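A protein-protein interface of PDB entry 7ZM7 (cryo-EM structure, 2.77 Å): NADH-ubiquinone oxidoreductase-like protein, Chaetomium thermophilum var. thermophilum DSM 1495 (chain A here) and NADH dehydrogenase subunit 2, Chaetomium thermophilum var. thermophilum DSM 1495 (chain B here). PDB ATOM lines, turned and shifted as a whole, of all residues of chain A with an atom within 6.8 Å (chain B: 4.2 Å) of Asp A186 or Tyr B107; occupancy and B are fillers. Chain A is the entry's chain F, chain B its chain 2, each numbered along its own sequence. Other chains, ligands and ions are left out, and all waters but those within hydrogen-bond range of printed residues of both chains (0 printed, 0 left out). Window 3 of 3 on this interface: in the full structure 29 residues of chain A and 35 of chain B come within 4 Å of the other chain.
OH of Tyr B108 sits close to NH1 of Arg A184, 3.4 Å away. The side-chain carboxylate (OD2) of Asp A186 sits close to the backbone carbonyl oxygen (O) of Tyr B107 (3.4 Å).
Among the printed residues, merely in contact across the chains: Glu A157 with Tyr B108, Asp A186 with Leu B106 and Lys A188 with Leu B106.
Asp A186 touches two residues of chain B. Tyr B107 touches just one residue of chain A: Asp A186 (3.2 Å). Of the printed residues of chain A, Tyr B108 touches Glu A157 and Arg A184. Printed residues of chain B within 4 Å of Glu A157: Tyr B108. Of the printed residues of chain A, Leu B106 touches Asp A186 (3.4 Å) and Lys A188 (3.9 Å). Of the printed residues of chain B, Lys A188 touches Leu B106 (3.9 Å). Leu B510 touches none of the printed residues of chain A. The nearest printed residue of chain B that does not touch Asp A186 is Tyr B108 (4.2 Å).
Hydrophobic or aromatic side chains of chain B that line the printed part of chain A: Leu B106 and Tyr B108. Among the printed residues, 5 pairs touch across the chains.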
ATOM      1  N   GLU A 122     -26.530  -3.162   1.491  1.00  0.00           N
ATOM      2  CA  GLU A 122     -25.816  -2.838   2.722  1.00  0.00           C
ATOM      3  C   GLU A 122     -24.400  -2.449   2.335  1.00  0.00           C
ATOM      4  O   GLU A 122     -23.492  -3.279   2.293  1.00  0.00           O
ATOM      5  CB  GLU A 122     -25.823  -4.017   3.684  1.00  0.00           C
ATOM      6  CG  GLU A 122     -27.180  -4.320   4.287  1.00  0.00           C
ATOM      7  CD  GLU A 122     -27.982  -5.271   3.428  1.00  0.00           C
ATOM      8  OE1 GLU A 122     -27.437  -5.754   2.413  1.00  0.00           O
ATOM      9  OE2 GLU A 122     -29.153  -5.535   3.764  1.00  0.00           O
ATOM     10  N   GLN A 124     -22.283  -0.876   3.980  1.00  0.00           N
ATOM     11  CA  GLN A 124     -21.325  -1.063   5.059  1.00  0.00           C
ATOM     12  C   GLN A 124     -20.855  -2.505   5.171  1.00  0.00           C
ATOM     13  O   GLN A 124     -19.956  -2.788   5.968  1.00  0.00           O
ATOM     14  CB  GLN A 124     -21.908  -0.615   6.405  1.00  0.00           C
ATOM     15  CG  GLN A 124     -23.044  -1.473   6.936  1.00  0.00           C
ATOM     16  CD  GLN A 124     -24.390  -0.785   6.849  1.00  0.00           C
ATOM     17  OE1 GLN A 124     -24.604   0.084   6.007  1.00  0.00           O
ATOM     18  NE2 GLN A 124     -25.306  -1.168   7.731  1.00  0.00           N
ATOM     19  N   GLU A 157     -23.570   3.095   8.363  1.00  0.00           N
ATOM     20  CA  GLU A 157     -24.883   2.767   7.830  1.00  0.00           C
ATOM     21  C   GLU A 157     -25.550   4.011   7.276  1.00  0.00           C
ATOM     22  O   GLU A 157     -25.682   5.017   7.976  1.00  0.00           O
ATOM     23  CB  GLU A 157     -25.777   2.139   8.893  1.00  0.00           C
ATOM     24  CG  GLU A 157     -27.171   1.876   8.344  1.00  0.00           C
ATOM     25  CD  GLU A 157     -28.014   0.949   9.174  1.00  0.00           C
ATOM     26  OE1 GLU A 157     -27.522   0.407  10.172  1.00  0.00           O
ATOM     27  OE2 GLU A 157     -29.186   0.769   8.816  1.00  0.00           O
ATOM     28  N   ARG A 184     -33.634  -6.189   4.545  1.00  0.00           N
ATOM     29  CA  ARG A 184     -32.243  -5.959   4.872  1.00  0.00           C
ATOM     30  C   ARG A 184     -31.798  -6.861   6.013  1.00  0.00           C
ATOM     31  O   ARG A 184     -32.594  -7.543   6.650  1.00  0.00           O
ATOM     32  CB  ARG A 184     -31.965  -4.506   5.260  1.00  0.00           C
ATOM     33  CG  ARG A 184     -32.096  -3.464   4.183  1.00  0.00           C
ATOM     34  CD  ARG A 184     -31.740  -2.134   4.806  1.00  0.00           C
ATOM     35  NE  ARG A 184     -31.780  -0.998   3.902  1.00  0.00           N
ATOM     36  CZ  ARG A 184     -32.842  -0.240   3.714  1.00  0.00           C
ATOM     37  NH1 ARG A 184     -33.930  -0.468   4.421  1.00  0.00           N
ATOM     38  NH2 ARG A 184     -32.802   0.778   2.869  1.00  0.00           N
ATOM     39  N   ARG A 185     -30.500  -6.829   6.286  1.00  0.00           N
ATOM     40  CA  ARG A 185     -29.922  -7.655   7.328  1.00  0.00           C
ATOM     41  C   ARG A 185     -28.970  -6.827   8.181  1.00  0.00           C
ATOM     42  O   ARG A 185     -28.410  -5.826   7.734  1.00  0.00           O
ATOM     43  CB  ARG A 185     -29.209  -8.870   6.727  1.00  0.00           C
ATOM     44  CG  ARG A 185     -28.016  -8.539   5.880  1.00  0.00           C
ATOM     45  CD  ARG A 185     -27.363  -9.805   5.354  1.00  0.00           C
ATOM     46  NE  ARG A 185     -26.249  -9.511   4.463  1.00  0.00           N
ATOM     47  CZ  ARG A 185     -25.000  -9.314   4.873  1.00  0.00           C
ATOM     48  NH1 ARG A 185     -24.708  -9.364   6.165  1.00  0.00           N
ATOM     49  NH2 ARG A 185     -24.043  -9.056   3.994  1.00  0.00           N
ATOM     50  N   ASP A 186     -28.822  -7.238   9.433  1.00  0.00           N
ATOM     51  CA  ASP A 186     -27.798  -6.660  10.289  1.00  0.00           C
ATOM     52  C   ASP A 186     -26.416  -6.960   9.725  1.00  0.00           C
ATOM     53  O   ASP A 186     -26.122  -8.089   9.331  1.00  0.00           O
ATOM     54  CB  ASP A 186     -27.910  -7.219  11.707  1.00  0.00           C
ATOM     55  CG  ASP A 186     -27.171  -6.375  12.724  1.00  0.00           C
ATOM     56  OD1 ASP A 186     -26.592  -5.342  12.322  1.00  0.00           O
ATOM     57  OD2 ASP A 186     -27.150  -6.746  13.918  1.00  0.00           O
ATOM     58  N   VAL A 187     -25.560  -5.939   9.691  1.00  0.00           N
ATOM     59  CA  VAL A 187     -24.243  -6.107   9.087  1.00  0.00           C
ATOM     60  C   VAL A 187     -23.444  -7.160   9.836  1.00  0.00           C
ATOM     61  O   VAL A 187     -22.595  -7.843   9.254  1.00  0.00           O
ATOM     62  CB  VAL A 187     -23.503  -4.757   9.035  1.00  0.00           C
ATOM     63  CG1 VAL A 187     -23.218  -4.249  10.435  1.00  0.00           C
ATOM     64  CG2 VAL A 187     -22.220  -4.883   8.233  1.00  0.00           C
ATOM     65  N   LYS A 188     -23.711  -7.320  11.131  1.00  0.00           N
ATOM     66  CA  LYS A 188     -23.059  -8.349  11.919  1.00  0.00           C
ATOM     67  C   LYS A 188     -23.652  -9.726  11.685  1.00  0.00           C
ATOM     68  O   LYS A 188     -23.018 -10.722  12.038  1.00  0.00           O
ATOM     69  CB  LYS A 188     -23.137  -7.973  13.399  1.00  0.00           C
ATOM     70  CG  LYS A 188     -22.317  -6.732  13.743  1.00  0.00           C
ATOM     71  CD  LYS A 188     -22.268  -6.458  15.238  1.00  0.00           C
ATOM     72  CE  LYS A 188     -23.589  -5.912  15.750  1.00  0.00           C
ATOM     73  NZ  LYS A 188     -23.515  -5.537  17.190  1.00  0.00           N
ATOM     74  N   ASP A 189     -24.834  -9.807  11.081  1.00  0.00           N
ATOM     75  CA  ASP A 189     -25.517 -11.076  10.835  1.00  0.00           C
ATOM     76  C   ASP A 189     -24.820 -11.801   9.689  1.00  0.00           C
ATOM     77  O   ASP A 189     -25.108 -11.587   8.513  1.00  0.00           O
ATOM     78  CB  ASP A 189     -26.988 -10.844  10.529  1.00  0.00           C
ATOM     79  CG  ASP A 189     -27.759 -12.135  10.372  1.00  0.00           C
ATOM     80  OD1 ASP A 189     -27.246 -13.192  10.791  1.00  0.00           O
ATOM     81  OD2 ASP A 189     -28.869 -12.101   9.804  1.00  0.00           O
ATOM     82  N   THR A 190     -23.894 -12.681  10.044  1.00  0.00           N
ATOM     83  CA  THR A 190     -23.147 -13.483   9.080  1.00  0.00           C
ATOM     84  C   THR A 190     -23.176 -14.944   9.535  1.00  0.00           C
ATOM     85  O   THR A 190     -22.239 -15.465  10.144  1.00  0.00           O
ATOM     86  CB  THR A 190     -21.714 -12.910   8.902  1.00  0.00           C
ATOM     87  OG1 THR A 190     -21.031 -13.597   7.845  1.00  0.00           O
ATOM     88  CG2 THR A 190     -20.903 -12.901  10.205  1.00  0.00           C
ATOM     89  N   VAL B  89     -37.732  -5.402  20.527  1.00  0.00           N
ATOM     90  CA  VAL B  89     -38.272  -6.680  19.998  1.00  0.00           C
ATOM     91  C   VAL B  89     -38.034  -7.706  21.101  1.00  0.00           C
ATOM     92  O   VAL B  89     -36.900  -7.793  21.569  1.00  0.00           O
ATOM     93  CB  VAL B  89     -37.590  -7.033  18.661  1.00  0.00           C
ATOM     94  CG1 VAL B  89     -37.544  -8.527  18.411  1.00  0.00           C
ATOM     95  CG2 VAL B  89     -38.219  -6.302  17.488  1.00  0.00           C
ATOM     96  N   LEU B 106     -29.387 -10.740  17.236  1.00  0.00           N
ATOM     97  CA  LEU B 106     -28.975  -9.918  16.070  1.00  0.00           C
ATOM     98  C   LEU B 106     -30.136  -9.815  15.078  1.00  0.00           C
ATOM     99  O   LEU B 106     -30.661 -10.865  14.705  1.00  0.00           O
ATOM    100  CB  LEU B 106     -27.802 -10.631  15.392  1.00  0.00           C
ATOM    101  CG  LEU B 106     -26.439 -10.438  16.053  1.00  0.00           C
ATOM    102  CD1 LEU B 106     -25.338 -11.037  15.194  1.00  0.00           C
ATOM    103  CD2 LEU B 106     -26.166  -8.963  16.302  1.00  0.00           C
ATOM    104  N   TYR B 107     -30.545  -8.609  14.681  1.00  0.00           N
ATOM    105  CA  TYR B 107     -31.554  -8.477  13.604  1.00  0.00           C
ATOM    106  C   TYR B 107     -31.359  -7.092  12.987  1.00  0.00           C
ATOM    107  O   TYR B 107     -30.495  -6.379  13.486  1.00  0.00           O
ATOM    108  CB  TYR B 107     -32.967  -8.685  14.154  1.00  0.00           C
ATOM    109  CG  TYR B 107     -33.459  -7.675  15.157  1.00  0.00           C
ATOM    110  CD1 TYR B 107     -33.081  -7.732  16.489  1.00  0.00           C
ATOM    111  CD2 TYR B 107     -34.348  -6.685  14.781  1.00  0.00           C
ATOM    112  CE1 TYR B 107     -33.553  -6.818  17.414  1.00  0.00           C
ATOM    113  CE2 TYR B 107     -34.831  -5.763  15.690  1.00  0.00           C
ATOM    114  CZ  TYR B 107     -34.431  -5.829  17.009  1.00  0.00           C
ATOM    115  OH  TYR B 107     -34.907  -4.912  17.895  1.00  0.00           O
ATOM    116  N   TYR B 108     -32.141  -6.714  11.979  1.00  0.00           N
ATOM    117  CA  TYR B 108     -32.014  -5.340  11.435  1.00  0.00           C
ATOM    118  C   TYR B 108     -32.795  -4.437  12.387  1.00  0.00           C
ATOM    119  O   TYR B 108     -34.019  -4.433  12.343  1.00  0.00           O
ATOM    120  CB  TYR B 108     -32.531  -5.309   9.995  1.00  0.00           C
ATOM    121  CG  TYR B 108     -32.510  -3.963   9.321  1.00  0.00           C
ATOM    122  CD1 TYR B 108     -31.381  -3.168   9.351  1.00  0.00           C
ATOM    123  CD2 TYR B 108     -33.612  -3.495   8.625  1.00  0.00           C
ATOM    124  CE1 TYR B 108     -31.352  -1.932   8.731  1.00  0.00           C
ATOM    125  CE2 TYR B 108     -33.606  -2.257   8.010  1.00  0.00           C
ATOM    126  CZ  TYR B 108     -32.470  -1.473   8.063  1.00  0.00           C
ATOM    127  OH  TYR B 108     -32.448  -0.254   7.453  1.00  0.00           O
ATOM    128  N   ARG B 109     -32.101  -3.720  13.262  1.00  0.00           N
ATOM    129  CA  ARG B 109     -32.841  -2.953  14.299  1.00  0.00           C
ATOM    130  C   ARG B 109     -33.157  -1.522  13.877  1.00  0.00           C
ATOM    131  O   ARG B 109     -34.040  -0.944  14.511  1.00  0.00           O
ATOM    132  CB  ARG B 109     -32.015  -2.916  15.589  1.00  0.00           C
ATOM    133  CG  ARG B 109     -31.533  -4.271  16.078  1.00  0.00           C
ATOM    134  CD  ARG B 109     -30.571  -4.038  17.218  1.00  0.00           C
ATOM    135  NE  ARG B 109     -30.490  -5.040  18.266  1.00  0.00           N
ATOM    136  CZ  ARG B 109     -31.059  -4.902  19.453  1.00  0.00           C
ATOM    137  NH1 ARG B 109     -31.747  -3.807  19.724  1.00  0.00           N
ATOM    138  NH2 ARG B 109     -30.931  -5.847  20.367  1.00  0.00           N
ATOM    139  N   ILE B 113     -36.339   0.304  15.675  1.00  0.00           N
ATOM    140  CA  ILE B 113     -36.033   1.094  16.868  1.00  0.00           C
ATOM    141  C   ILE B 113     -35.847   2.575  16.575  1.00  0.00           C
ATOM    142  O   ILE B 113     -35.598   3.343  17.510  1.00  0.00           O
ATOM    143  CB  ILE B 113     -34.786   0.558  17.609  1.00  0.00           C
ATOM    144  CG1 ILE B 113     -33.502   0.897  16.846  1.00  0.00           C
ATOM    145  CG2 ILE B 113     -34.912  -0.928  17.931  1.00  0.00           C
ATOM    146  CD1 ILE B 113     -32.256   0.403  17.491  1.00  0.00           C
ATOM    147  N   PHE B 508     -39.243 -10.882   9.768  1.00  0.00           N
ATOM    148  CA  PHE B 508     -37.818 -10.482   9.875  1.00  0.00           C
ATOM    149  C   PHE B 508     -37.080 -11.576  10.652  1.00  0.00           C
ATOM    150  O   PHE B 508     -37.599 -12.038  11.681  1.00  0.00           O
ATOM    151  CB  PHE B 508     -37.654  -9.047  10.386  1.00  0.00           C
ATOM    152  CG  PHE B 508     -38.146  -8.756  11.781  1.00  0.00           C
ATOM    153  CD1 PHE B 508     -37.313  -8.921  12.876  1.00  0.00           C
ATOM    154  CD2 PHE B 508     -39.425  -8.268  11.994  1.00  0.00           C
ATOM    155  CE1 PHE B 508     -37.758  -8.630  14.154  1.00  0.00           C
ATOM    156  CE2 PHE B 508     -39.869  -7.982  13.273  1.00  0.00           C
ATOM    157  CZ  PHE B 508     -39.036  -8.163  14.350  1.00  0.00           C
ATOM    158  N   SER B 509     -35.923 -11.997  10.152  1.00  0.00           N
ATOM    159  CA  SER B 509     -35.187 -13.116  10.785  1.00  0.00           C
ATOM    160  C   SER B 509     -34.348 -12.614  11.965  1.00  0.00           C
ATOM    161  O   SER B 509     -33.554 -11.676  11.771  1.00  0.00           O
ATOM    162  CB  SER B 509     -34.327 -13.794   9.756  1.00  0.00           C
ATOM    163  OG  SER B 509     -33.447 -12.866   9.140  1.00  0.00           O
ATOM    164  N   LEU B 510     -34.536 -13.210  13.146  1.00  0.00           N
ATOM    165  CA  LEU B 510     -33.736 -12.818  14.324  1.00  0.00           C
ATOM    166  C   LEU B 510     -32.810 -13.974  14.701  1.00  0.00           C
ATOM    167  O   LEU B 510     -33.297 -15.108  14.798  1.00  0.00           O
ATOM    168  CB  LEU B 510     -34.669 -12.405  15.463  1.00  0.00           C
ATOM    169  CG  LEU B 510     -33.983 -11.957  16.751  1.00  0.00           C
ATOM    170  CD1 LEU B 510     -34.725 -10.792  17.378  1.00  0.00           C
ATOM    171  CD2 LEU B 510     -33.883 -13.108  17.734  1.00  0.00           C
